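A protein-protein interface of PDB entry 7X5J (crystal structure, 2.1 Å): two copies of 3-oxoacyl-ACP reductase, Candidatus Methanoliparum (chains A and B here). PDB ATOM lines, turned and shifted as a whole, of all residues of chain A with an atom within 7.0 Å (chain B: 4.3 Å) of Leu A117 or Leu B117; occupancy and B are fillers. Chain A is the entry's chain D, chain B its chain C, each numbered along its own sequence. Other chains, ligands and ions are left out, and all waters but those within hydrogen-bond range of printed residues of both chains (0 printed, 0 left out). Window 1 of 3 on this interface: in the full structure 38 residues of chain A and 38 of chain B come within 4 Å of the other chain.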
ATOM      1  N   ALA A  91      31.103  26.266  18.501  1.00  0.00           N
ATOM      2  CA  ALA A  91      30.135  26.861  17.544  1.00  0.00           C
ATOM      3  C   ALA A  91      29.181  25.771  17.027  1.00  0.00           C
ATOM      4  O   ALA A  91      29.691  24.702  16.605  1.00  0.00           O
ATOM      5  CB  ALA A  91      30.862  27.529  16.401  1.00  0.00           C
ATOM      6  N   TRP A 109      19.421  21.729   6.915  1.00  0.00           N
ATOM      7  CA  TRP A 109      20.264  20.522   7.106  1.00  0.00           C
ATOM      8  C   TRP A 109      21.716  20.815   6.692  1.00  0.00           C
ATOM      9  O   TRP A 109      22.610  20.670   7.549  1.00  0.00           O
ATOM     10  CB  TRP A 109      19.664  19.353   6.330  1.00  0.00           C
ATOM     11  CG  TRP A 109      20.570  18.173   6.189  1.00  0.00           C
ATOM     12  CD1 TRP A 109      21.493  17.944   5.210  1.00  0.00           C
ATOM     13  CD2 TRP A 109      20.609  17.032   7.054  1.00  0.00           C
ATOM     14  NE1 TRP A 109      22.103  16.733   5.410  1.00  0.00           N
ATOM     15  CE2 TRP A 109      21.588  16.159   6.542  1.00  0.00           C
ATOM     16  CE3 TRP A 109      19.924  16.675   8.216  1.00  0.00           C
ATOM     17  CZ2 TRP A 109      21.879  14.939   7.148  1.00  0.00           C
ATOM     18  CZ3 TRP A 109      20.208  15.470   8.810  1.00  0.00           C
ATOM     19  CH2 TRP A 109      21.177  14.617   8.282  1.00  0.00           C
ATOM     20  N   GLN A 111      23.359  23.516   6.285  1.00  0.00           N
ATOM     21  CA  GLN A 111      23.992  24.606   7.072  1.00  0.00           C
ATOM     22  C   GLN A 111      24.469  24.025   8.408  1.00  0.00           C
ATOM     23  O   GLN A 111      25.653  24.187   8.737  1.00  0.00           O
ATOM     24  CB  GLN A 111      22.998  25.753   7.227  1.00  0.00           C
ATOM     25  CG  GLN A 111      23.557  26.966   7.954  1.00  0.00           C
ATOM     26  CD  GLN A 111      22.441  27.870   8.418  1.00  0.00           C
ATOM     27  OE1 GLN A 111      21.664  28.406   7.620  1.00  0.00           O
ATOM     28  NE2 GLN A 111      22.343  28.032   9.728  1.00  0.00           N
ATOM     29  N   ASP A 112      23.572  23.333   9.110  1.00  0.00           N
ATOM     30  CA  ASP A 112      23.836  22.547  10.347  1.00  0.00           C
ATOM     31  C   ASP A 112      25.051  21.632  10.148  1.00  0.00           C
ATOM     32  O   ASP A 112      25.921  21.648  11.025  1.00  0.00           O
ATOM     33  CB  ASP A 112      22.588  21.759  10.752  1.00  0.00           C
ATOM     34  CG  ASP A 112      21.440  22.639  11.237  1.00  0.00           C
ATOM     35  OD1 ASP A 112      21.658  23.852  11.398  1.00  0.00           O
ATOM     36  OD2 ASP A 112      20.344  22.094  11.470  1.00  0.00           O
ATOM     37  N   LEU A 113      25.141  20.911   9.026  1.00  0.00           N
ATOM     38  CA  LEU A 113      26.298  20.014   8.744  1.00  0.00           C
ATOM     39  C   LEU A 113      27.569  20.854   8.528  1.00  0.00           C
ATOM     40  O   LEU A 113      28.615  20.486   9.126  1.00  0.00           O
ATOM     41  CB  LEU A 113      26.005  19.095   7.547  1.00  0.00           C
ATOM     42  CG  LEU A 113      25.447  17.721   7.927  1.00  0.00           C
ATOM     43  CD1 LEU A 113      24.073  17.851   8.577  1.00  0.00           C
ATOM     44  CD2 LEU A 113      25.379  16.805   6.728  1.00  0.00           C
ATOM     45  N   ARG A 114      27.499  21.924   7.716  1.00  0.00           N
ATOM     46  CA  ARG A 114      28.668  22.803   7.380  1.00  0.00           C
ATOM     47  C   ARG A 114      29.250  23.408   8.665  1.00  0.00           C
ATOM     48  O   ARG A 114      30.497  23.469   8.815  1.00  0.00           O
ATOM     49  CB  ARG A 114      28.282  23.942   6.426  1.00  0.00           C
ATOM     50  CG  ARG A 114      28.314  23.571   4.948  1.00  0.00           C
ATOM     51  CD  ARG A 114      28.139  24.797   4.062  1.00  0.00           C
ATOM     52  NE  ARG A 114      27.164  25.755   4.596  1.00  0.00           N
ATOM     53  CZ  ARG A 114      25.879  25.854   4.228  1.00  0.00           C
ATOM     54  NH1 ARG A 114      25.375  25.048   3.304  1.00  0.00           N
ATOM     55  NH2 ARG A 114      25.106  26.769   4.798  1.00  0.00           N
ATOM     56  N   VAL A 115      28.383  23.834   9.575  1.00  0.00           N
ATOM     57  CA  VAL A 115      28.824  24.503  10.825  1.00  0.00           C
ATOM     58  C   VAL A 115      29.314  23.444  11.827  1.00  0.00           C
ATOM     59  O   VAL A 115      30.417  23.619  12.396  1.00  0.00           O
ATOM     60  CB  VAL A 115      27.701  25.383  11.402  1.00  0.00           C
ATOM     61  CG1 VAL A 115      28.121  26.008  12.722  1.00  0.00           C
ATOM     62  CG2 VAL A 115      27.276  26.457  10.411  1.00  0.00           C
ATOM     63  N   ASN A 116      28.524  22.392  12.062  1.00  0.00           N
ATOM     64  CA  ASN A 116      28.743  21.481  13.215  1.00  0.00           C
ATOM     65  C   ASN A 116      29.842  20.468  12.892  1.00  0.00           C
ATOM     66  O   ASN A 116      30.611  20.128  13.817  1.00  0.00           O
ATOM     67  CB  ASN A 116      27.432  20.829  13.614  1.00  0.00           C
ATOM     68  CG  ASN A 116      26.396  21.865  13.975  1.00  0.00           C
ATOM     69  OD1 ASN A 116      26.693  23.059  14.021  1.00  0.00           O
ATOM     70  ND2 ASN A 116      25.185  21.414  14.219  1.00  0.00           N
ATOM     71  N   LEU A 117      29.944  20.044  11.631  1.00  0.00           N
ATOM     72  CA  LEU A 117      30.960  19.050  11.210  1.00  0.00           C
ATOM     73  C   LEU A 117      32.117  19.746  10.476  1.00  0.00           C
ATOM     74  O   LEU A 117      33.284  19.624  10.955  1.00  0.00           O
ATOM     75  CB  LEU A 117      30.271  17.953  10.385  1.00  0.00           C
ATOM     76  CG  LEU A 117      29.274  17.119  11.189  1.00  0.00           C
ATOM     77  CD1 LEU A 117      28.642  16.017  10.346  1.00  0.00           C
ATOM     78  CD2 LEU A 117      29.953  16.548  12.421  1.00  0.00           C
ATOM     79  N   THR A 118      31.844  20.469   9.384  1.00  0.00           N
ATOM     80  CA  THR A 118      32.919  21.121   8.588  1.00  0.00           C
ATOM     81  C   THR A 118      33.642  22.166   9.441  1.00  0.00           C
ATOM     82  O   THR A 118      34.863  22.281   9.295  1.00  0.00           O
ATOM     83  CB  THR A 118      32.400  21.628   7.244  1.00  0.00           C
ATOM     84  OG1 THR A 118      31.587  20.557   6.776  1.00  0.00           O
ATOM     85  CG2 THR A 118      33.512  21.927   6.261  1.00  0.00           C
ATOM     86  N   GLY A 119      32.941  22.834  10.352  1.00  0.00           N
ATOM     87  CA  GLY A 119      33.564  23.752  11.322  1.00  0.00           C
ATOM     88  C   GLY A 119      34.666  23.071  12.118  1.00  0.00           C
ATOM     89  O   GLY A 119      35.818  23.550  12.075  1.00  0.00           O
ATOM     90  N   ALA A 120      34.332  21.974  12.802  1.00  0.00           N
ATOM     91  CA  ALA A 120      35.282  21.170  13.602  1.00  0.00           C
ATOM     92  C   ALA A 120      36.446  20.736  12.705  1.00  0.00           C
ATOM     93  O   ALA A 120      37.601  20.866  13.133  1.00  0.00           O
ATOM     94  CB  ALA A 120      34.568  19.986  14.217  1.00  0.00           C
ATOM     95  N   PHE A 121      36.147  20.232  11.502  1.00  0.00           N
ATOM     96  CA  PHE A 121      37.157  19.784  10.508  1.00  0.00           C
ATOM     97  C   PHE A 121      38.110  20.944  10.199  1.00  0.00           C
ATOM     98  O   PHE A 121      39.323  20.800  10.398  1.00  0.00           O
ATOM     99  CB  PHE A 121      36.454  19.273   9.259  1.00  0.00           C
ATOM    100  CG  PHE A 121      37.317  19.025   8.047  1.00  0.00           C
ATOM    101  CD1 PHE A 121      37.978  17.814   7.881  1.00  0.00           C
ATOM    102  CD2 PHE A 121      37.384  19.964   7.023  1.00  0.00           C
ATOM    103  CE1 PHE A 121      38.719  17.562   6.738  1.00  0.00           C
ATOM    104  CE2 PHE A 121      38.110  19.705   5.873  1.00  0.00           C
ATOM    105  CZ  PHE A 121      38.784  18.509   5.736  1.00  0.00           C
ATOM    106  N   ASN A 122      37.561  22.078   9.763  1.00  0.00           N
ATOM    107  CA  ASN A 122      38.351  23.247   9.289  1.00  0.00           C
ATOM    108  C   ASN A 122      39.270  23.721  10.423  1.00  0.00           C
ATOM    109  O   ASN A 122      40.489  23.938  10.167  1.00  0.00           O
ATOM    110  CB  ASN A 122      37.450  24.372   8.774  1.00  0.00           C
ATOM    111  CG  ASN A 122      36.856  24.110   7.401  1.00  0.00           C
ATOM    112  OD1 ASN A 122      37.397  23.347   6.596  1.00  0.00           O
ATOM    113  ND2 ASN A 122      35.747  24.770   7.113  1.00  0.00           N
ATOM    114  N   CYS A 123      38.729  23.873  11.633  1.00  0.00           N
ATOM    115  CA  CYS A 123      39.508  24.388  12.785  1.00  0.00           C
ATOM    116  C   CYS A 123      40.614  23.387  13.135  1.00  0.00           C
ATOM    117  O   CYS A 123      41.766  23.819  13.248  1.00  0.00           O
ATOM    118  CB  CYS A 123      38.608  24.668  13.974  1.00  0.00           C
ATOM    119  SG  CYS A 123      37.408  25.976  13.626  1.00  0.00           S
ATOM    120  N   ILE A 124      40.285  22.093  13.253  1.00  0.00           N
ATOM    121  CA  ILE A 124      41.299  21.051  13.579  1.00  0.00           C
ATOM    122  C   ILE A 124      42.371  21.065  12.476  1.00  0.00           C
ATOM    123  O   ILE A 124      43.554  20.940  12.801  1.00  0.00           O
ATOM    124  CB  ILE A 124      40.661  19.658  13.788  1.00  0.00           C
ATOM    125  CG1 ILE A 124      39.778  19.597  15.040  1.00  0.00           C
ATOM    126  CG2 ILE A 124      41.735  18.577  13.832  1.00  0.00           C
ATOM    127  CD1 ILE A 124      38.787  18.427  15.048  1.00  0.00           C
ATOM    128  N   SER A 156      19.274  16.835  12.080  1.00  0.00           N
ATOM    129  CA  SER A 156      20.595  17.429  11.754  1.00  0.00           C
ATOM    130  C   SER A 156      21.437  17.534  13.030  1.00  0.00           C
ATOM    131  O   SER A 156      22.674  17.338  12.968  1.00  0.00           O
ATOM    132  CB  SER A 156      20.448  18.785  11.126  1.00  0.00           C
ATOM    133  OG  SER A 156      20.277  19.783  12.134  1.00  0.00           O
ATOM    134  N   THR A 159      22.419  14.014  14.141  1.00  0.00           N
ATOM    135  CA  THR A 159      23.383  13.501  13.139  1.00  0.00           C
ATOM    136  C   THR A 159      24.753  14.127  13.412  1.00  0.00           C
ATOM    137  O   THR A 159      25.750  13.381  13.395  1.00  0.00           O
ATOM    138  CB  THR A 159      22.921  13.729  11.701  1.00  0.00           C
ATOM    139  OG1 THR A 159      21.693  13.019  11.547  1.00  0.00           O
ATOM    140  CG2 THR A 159      23.924  13.224  10.689  1.00  0.00           C
ATOM    141  N   THR A 160      24.806  15.436  13.658  1.00  0.00           N
ATOM    142  CA  THR A 160      26.081  16.182  13.668  1.00  0.00           C
ATOM    143  C   THR A 160      26.756  15.943  15.010  1.00  0.00           C
ATOM    144  O   THR A 160      27.979  15.809  15.031  1.00  0.00           O
ATOM    145  CB  THR A 160      25.902  17.672  13.343  1.00  0.00           C
ATOM    146  OG1 THR A 160      24.997  18.303  14.254  1.00  0.00           O
ATOM    147  CG2 THR A 160      25.478  17.887  11.903  1.00  0.00           C
ATOM    148  N   LYS A 161      25.973  15.899  16.082  1.00  0.00           N
ATOM    149  CA  LYS A 161      26.501  15.725  17.456  1.00  0.00           C
ATOM    150  C   LYS A 161      27.046  14.303  17.595  1.00  0.00           C
ATOM    151  O   LYS A 161      28.057  14.143  18.292  1.00  0.00           O
ATOM    152  CB  LYS A 161      25.428  16.108  18.477  1.00  0.00           C
ATOM    153  CG  LYS A 161      25.048  17.584  18.424  1.00  0.00           C
ATOM    154  CD  LYS A 161      26.116  18.513  18.952  1.00  0.00           C
ATOM    155  CE  LYS A 161      26.396  19.664  18.020  1.00  0.00           C
ATOM    156  NZ  LYS A 161      27.234  20.694  18.672  1.00  0.00           N
ATOM    157  N   ALA A 162      26.450  13.329  16.903  1.00  0.00           N
ATOM    158  CA  ALA A 162      26.947  11.934  16.871  1.00  0.00           C
ATOM    159  C   ALA A 162      28.218  11.886  16.024  1.00  0.00           C
ATOM    160  O   ALA A 162      29.151  11.207  16.423  1.00  0.00           O
ATOM    161  CB  ALA A 162      25.896  10.981  16.352  1.00  0.00           C
ATOM    162  N   GLY A 163      28.219  12.544  14.867  1.00  0.00           N
ATOM    163  CA  GLY A 163      29.355  12.573  13.926  1.00  0.00           C
ATOM    164  C   GLY A 163      30.601  13.141  14.583  1.00  0.00           C
ATOM    165  O   GLY A 163      31.725  12.635  14.293  1.00  0.00           O
ATOM    166  N   LEU A 164      30.432  14.143  15.451  1.00  0.00           N
ATOM    167  CA  LEU A 164      31.572  14.749  16.195  1.00  0.00           C
ATOM    168  C   LEU A 164      32.249  13.702  17.086  1.00  0.00           C
ATOM    169  O   LEU A 164      33.454  13.835  17.323  1.00  0.00           O
ATOM    170  CB  LEU A 164      31.084  15.955  17.000  1.00  0.00           C
ATOM    171  CG  LEU A 164      30.912  17.228  16.177  1.00  0.00           C
ATOM    172  CD1 LEU A 164      30.222  18.295  17.005  1.00  0.00           C
ATOM    173  CD2 LEU A 164      32.260  17.723  15.655  1.00  0.00           C
ATOM    174  N   ILE A 165      31.553  12.652  17.517  1.00  0.00           N
ATOM    175  CA  ILE A 165      32.196  11.582  18.346  1.00  0.00           C
ATOM    176  C   ILE A 165      33.096  10.728  17.439  1.00  0.00           C
ATOM    177  O   ILE A 165      34.278  10.485  17.806  1.00  0.00           O
ATOM    178  CB  ILE A 165      31.142  10.783  19.123  1.00  0.00           C
ATOM    179  CG1 ILE A 165      30.408  11.711  20.099  1.00  0.00           C
ATOM    180  CG2 ILE A 165      31.754   9.563  19.819  1.00  0.00           C
ATOM    181  CD1 ILE A 165      29.226  11.060  20.780  1.00  0.00           C
ATOM    182  N   LEU A 167      34.495  11.802  14.664  1.00  0.00           N
ATOM    183  CA  LEU A 167      35.608  12.727  14.304  1.00  0.00           C
ATOM    184  C   LEU A 167      36.625  12.757  15.455  1.00  0.00           C
ATOM    185  O   LEU A 167      37.852  12.699  15.192  1.00  0.00           O
ATOM    186  CB  LEU A 167      35.050  14.128  14.039  1.00  0.00           C
ATOM    187  CG  LEU A 167      36.102  15.204  13.809  1.00  0.00           C
ATOM    188  CD1 LEU A 167      36.890  14.916  12.546  1.00  0.00           C
ATOM    189  CD2 LEU A 167      35.465  16.573  13.749  1.00  0.00           C
ATOM    190  N   TRP B 109      36.076  15.802   1.773  1.00  0.00           N
ATOM    191  CA  TRP B 109      35.241  15.862   3.004  1.00  0.00           C
ATOM    192  C   TRP B 109      33.794  16.179   2.619  1.00  0.00           C
ATOM    193  O   TRP B 109      32.901  15.409   3.007  1.00  0.00           O
ATOM    194  CB  TRP B 109      35.797  16.899   3.974  1.00  0.00           C
ATOM    195  CG  TRP B 109      34.950  17.188   5.177  1.00  0.00           C
ATOM    196  CD1 TRP B 109      34.052  18.200   5.304  1.00  0.00           C
ATOM    197  CD2 TRP B 109      34.993  16.532   6.458  1.00  0.00           C
ATOM    198  NE1 TRP B 109      33.514  18.208   6.560  1.00  0.00           N
ATOM    199  CE2 TRP B 109      34.064  17.189   7.288  1.00  0.00           C
ATOM    200  CE3 TRP B 109      35.694  15.438   6.980  1.00  0.00           C
ATOM    201  CZ2 TRP B 109      33.826  16.797   8.608  1.00  0.00           C
ATOM    202  CZ3 TRP B 109      35.454  15.044   8.278  1.00  0.00           C
ATOM    203  CH2 TRP B 109      34.541  15.724   9.084  1.00  0.00           C
ATOM    204  N   ASP B 112      31.854  13.361   0.757  1.00  0.00           N
ATOM    205  CA  ASP B 112      31.640  12.240   1.705  1.00  0.00           C
ATOM    206  C   ASP B 112      30.403  12.571   2.552  1.00  0.00           C
ATOM    207  O   ASP B 112      29.519  11.691   2.682  1.00  0.00           O
ATOM    208  CB  ASP B 112      32.923  11.985   2.499  1.00  0.00           C
ATOM    209  CG  ASP B 112      34.070  11.454   1.652  1.00  0.00           C
ATOM    210  OD1 ASP B 112      33.809  11.058   0.512  1.00  0.00           O
ATOM    211  OD2 ASP B 112      35.218  11.420   2.147  1.00  0.00           O
ATOM    212  N   LEU B 113      30.290  13.814   3.030  1.00  0.00           N
ATOM    213  CA  LEU B 113      29.159  14.244   3.889  1.00  0.00           C
ATOM    214  C   LEU B 113      27.867  14.305   3.066  1.00  0.00           C
ATOM    215  O   LEU B 113      26.835  13.889   3.602  1.00  0.00           O
ATOM    216  CB  LEU B 113      29.479  15.572   4.579  1.00  0.00           C
ATOM    217  CG  LEU B 113      30.029  15.457   6.005  1.00  0.00           C
ATOM    218  CD1 LEU B 113      31.407  14.799   6.027  1.00  0.00           C
ATOM    219  CD2 LEU B 113      30.097  16.808   6.696  1.00  0.00           C
ATOM    220  N   VAL B 115      27.035  12.556   0.249  1.00  0.00           N
ATOM    221  CA  VAL B 115      26.638  11.160  -0.094  1.00  0.00           C
ATOM    222  C   VAL B 115      26.193  10.426   1.181  1.00  0.00           C
ATOM    223  O   VAL B 115      25.060   9.898   1.178  1.00  0.00           O
ATOM    224  CB  VAL B 115      27.763  10.395  -0.816  1.00  0.00           C
ATOM    225  CG1 VAL B 115      27.328   8.974  -1.131  1.00  0.00           C
ATOM    226  CG2 VAL B 115      28.214  11.108  -2.088  1.00  0.00           C
ATOM    227  N   ASN B 116      27.042  10.400   2.219  1.00  0.00           N
ATOM    228  CA  ASN B 116      26.931   9.452   3.362  1.00  0.00           C
ATOM    229  C   ASN B 116      25.871   9.925   4.356  1.00  0.00           C
ATOM    230  O   ASN B 116      25.119   9.055   4.847  1.00  0.00           O
ATOM    231  CB  ASN B 116      28.279   9.191   4.033  1.00  0.00           C
ATOM    232  CG  ASN B 116      29.310   8.611   3.085  1.00  0.00           C
ATOM    233  OD1 ASN B 116      29.043   8.447   1.895  1.00  0.00           O
ATOM    234  ND2 ASN B 116      30.493   8.293   3.594  1.00  0.00           N
ATOM    235  N   LEU B 117      25.784  11.225   4.637  1.00  0.00           N
ATOM    236  CA  LEU B 117      24.742  11.789   5.540  1.00  0.00           C
ATOM    237  C   LEU B 117      23.544  12.297   4.728  1.00  0.00           C
ATOM    238  O   LEU B 117      22.465  11.725   4.866  1.00  0.00           O
ATOM    239  CB  LEU B 117      25.356  12.888   6.408  1.00  0.00           C
ATOM    240  CG  LEU B 117      26.434  12.404   7.385  1.00  0.00           C
ATOM    241  CD1 LEU B 117      26.951  13.558   8.248  1.00  0.00           C
ATOM    242  CD2 LEU B 117      25.922  11.266   8.267  1.00  0.00           C
ATOM    243  N   THR B 118      23.722  13.313   3.888  1.00  0.00           N
ATOM    244  CA  THR B 118      22.617  14.004   3.161  1.00  0.00           C
ATOM    245  C   THR B 118      21.921  13.011   2.215  1.00  0.00           C
ATOM    246  O   THR B 118      20.703  13.127   2.033  1.00  0.00           O
ATOM    247  CB  THR B 118      23.137  15.252   2.434  1.00  0.00           C
ATOM    248  OG1 THR B 118      24.096  15.884   3.280  1.00  0.00           O
ATOM    249  CG2 THR B 118      22.031  16.217   2.070  1.00  0.00           C
ATOM    250  N   GLY B 119      22.660  12.062   1.649  1.00  0.00           N
ATOM    251  CA  GLY B 119      22.079  10.936   0.890  1.00  0.00           C
ATOM    252  C   GLY B 119      21.014  10.217   1.706  1.00  0.00           C
ATOM    253  O   GLY B 119      19.899  10.019   1.178  1.00  0.00           O
ATOM    254  N   ALA B 120      21.327   9.885   2.966  1.00  0.00           N
ATOM    255  CA  ALA B 120      20.425   9.131   3.866  1.00  0.00           C
ATOM    256  C   ALA B 120      19.243  10.029   4.236  1.00  0.00           C
ATOM    257  O   ALA B 120      18.103   9.566   4.105  1.00  0.00           O
ATOM    258  CB  ALA B 120      21.176   8.631   5.080  1.00  0.00           C
ATOM    259  N   PHE B 121      19.516  11.272   4.639  1.00  0.00           N
ATOM    260  CA  PHE B 121      18.491  12.323   4.892  1.00  0.00           C
ATOM    261  C   PHE B 121      17.535  12.474   3.688  1.00  0.00           C
ATOM    262  O   PHE B 121      16.313  12.395   3.872  1.00  0.00           O
ATOM    263  CB  PHE B 121      19.194  13.627   5.240  1.00  0.00           C
ATOM    264  CG  PHE B 121      18.317  14.851   5.199  1.00  0.00           C
ATOM    265  CD1 PHE B 121      17.495  15.171   6.266  1.00  0.00           C
ATOM    266  CD2 PHE B 121      18.340  15.702   4.101  1.00  0.00           C
ATOM    267  CE1 PHE B 121      16.702  16.310   6.230  1.00  0.00           C
ATOM    268  CE2 PHE B 121      17.561  16.850   4.075  1.00  0.00           C
ATOM    269  CZ  PHE B 121      16.753  17.156   5.143  1.00  0.00           C
ATOM    270  N   THR B 159      33.429  10.206  10.728  1.00  0.00           N
ATOM    271  CA  THR B 159      32.420  11.256  11.056  1.00  0.00           C
ATOM    272  C   THR B 159      31.056  10.812  10.511  1.00  0.00           C
ATOM    273  O   THR B 159      30.072  10.876  11.264  1.00  0.00           O
ATOM    274  CB  THR B 159      32.792  12.645  10.509  1.00  0.00           C
ATOM    275  OG1 THR B 159      34.062  13.054  11.018  1.00  0.00           O
ATOM    276  CG2 THR B 159      31.776  13.705  10.872  1.00  0.00           C
ATOM    277  N   THR B 160      30.978  10.435   9.236  1.00  0.00           N
ATOM    278  CA  THR B 160      29.675  10.182   8.562  1.00  0.00           C
ATOM    279  C   THR B 160      29.070   8.891   9.143  1.00  0.00           C
ATOM    280  O   THR B 160      27.869   8.872   9.412  1.00  0.00           O
ATOM    281  CB  THR B 160      29.828  10.218   7.035  1.00  0.00           C
ATOM    282  OG1 THR B 160      30.803   9.276   6.593  1.00  0.00           O
ATOM    283  CG2 THR B 160      30.207  11.594   6.530  1.00  0.00           C
ATOM    284  N   GLY B 163      27.809   9.616  12.449  1.00  0.00           N
ATOM    285  CA  GLY B 163      26.673  10.542  12.299  1.00  0.00           C
ATOM    286  C   GLY B 163      25.388   9.788  12.007  1.00  0.00           C
ATOM    287  O   GLY B 163      24.334  10.196  12.506  1.00  0.00           O
ATOM    288  N   LEU B 164      25.495   8.729  11.209  1.00  0.00           N
ATOM    289  CA  LEU B 164      24.372   7.855  10.807  1.00  0.00           C
ATOM    290  C   LEU B 164      23.730   7.167  12.024  1.00  0.00           C
ATOM    291  O   LEU B 164      22.515   6.903  11.976  1.00  0.00           O
ATOM    292  CB  LEU B 164      24.896   6.846   9.788  1.00  0.00           C
ATOM    293  CG  LEU B 164      25.045   7.400   8.373  1.00  0.00           C
ATOM    294  CD1 LEU B 164      25.815   6.416   7.501  1.00  0.00           C
ATOM    295  CD2 LEU B 164      23.686   7.702   7.757  1.00  0.00           C
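N of Thr B118 lies within hydrogen-bond range of O of Leu B113 (3.2 Å). O of Leu A113 sits at hydrogen-bond distance from N of Thr A118. The backbone carbonyl oxygen of Thr A118 lies close to the side-chain amide nitrogen of Asn A122, at 3.4 Å.
OG1 of Thr A118 is in hydrogen-bond range of NE1 of Trp B109, 3.0 Å away. The indole nitrogen of Trp A109 is in hydrogen-bond range of the side-chain hydroxyl of Thr B118 (3.0 Å).
Trp A109 touches Thr B118, and with the chains exchanged Thr A118 touches Trp B109. Trp A109 touches Phe B121, and with the chains exchanged Phe A121 touches Trp B109. Leu A113 touches Thr B118, but with the chains exchanged Thr A118 does not touch Leu B113 (4.04 Å). Leu A117 touches Thr B159, and with the chains exchanged Thr A159 touches Leu B117. 14 positions are printed for both chains. Of the 16 pairs that touch across the chains among the printed residues, 14 have their exchanged pair printed and touching as well.
Leu B117 touches Trp A109. Trp A109 touches Phe B121. OG1 of Thr B118 touches CD2 of Leu A113, at 3.8 Å. Trp B109 touches Leu A117. Leu B117 touches Leu A117 (CD1 to CD1, 3.6 Å). Thr B159 touches Leu A117. Trp B109 touches Phe A121. Gly B163 touches Thr A159 (CA to O, 3.2 Å). CA of Gly B163 touches N of Gly A163, at 3.6 Å. CB of Leu A167 touches OG1 of Thr B159, at 3.4 Å.
Printed residues of chain A that touch a printed residue of chain B: Trp A109, Leu A113, Leu A117, Thr A118, Phe A121, Thr A159, Gly A163 and Leu A167. Hydrophobic or aromatic side chains of chain A that line the printed part of chain B: Trp A109, Leu A113, Leu A117, Phe A121 and Leu A167. Of the 14 printed residues of chain B, 7 touch a printed residue of chain A. Hydrophobic or aromatic side chains of chain B that line the printed part of chain A: Trp B109, Leu B113, Leu B117 and Phe B121.
Printed residues of chain A within 4 Å of Leu B117: Trp A109 (3.95 Å), Leu A113 (3.9 Å), Leu A117 (3.6 Å) and Thr A159 (3.7 Å). Printed residues of chain A within 4 Å of Gly B163: Thr A159 (3.2 Å) and Gly A163 (3.6 Å). Printed residues of chain B within 4 Å of Leu A113: Leu B117 (3.9 Å) and Thr B118 (3.8 Å). Printed residues of chain B within 4 Å of Leu A167: Thr B159 (3.4 Å).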
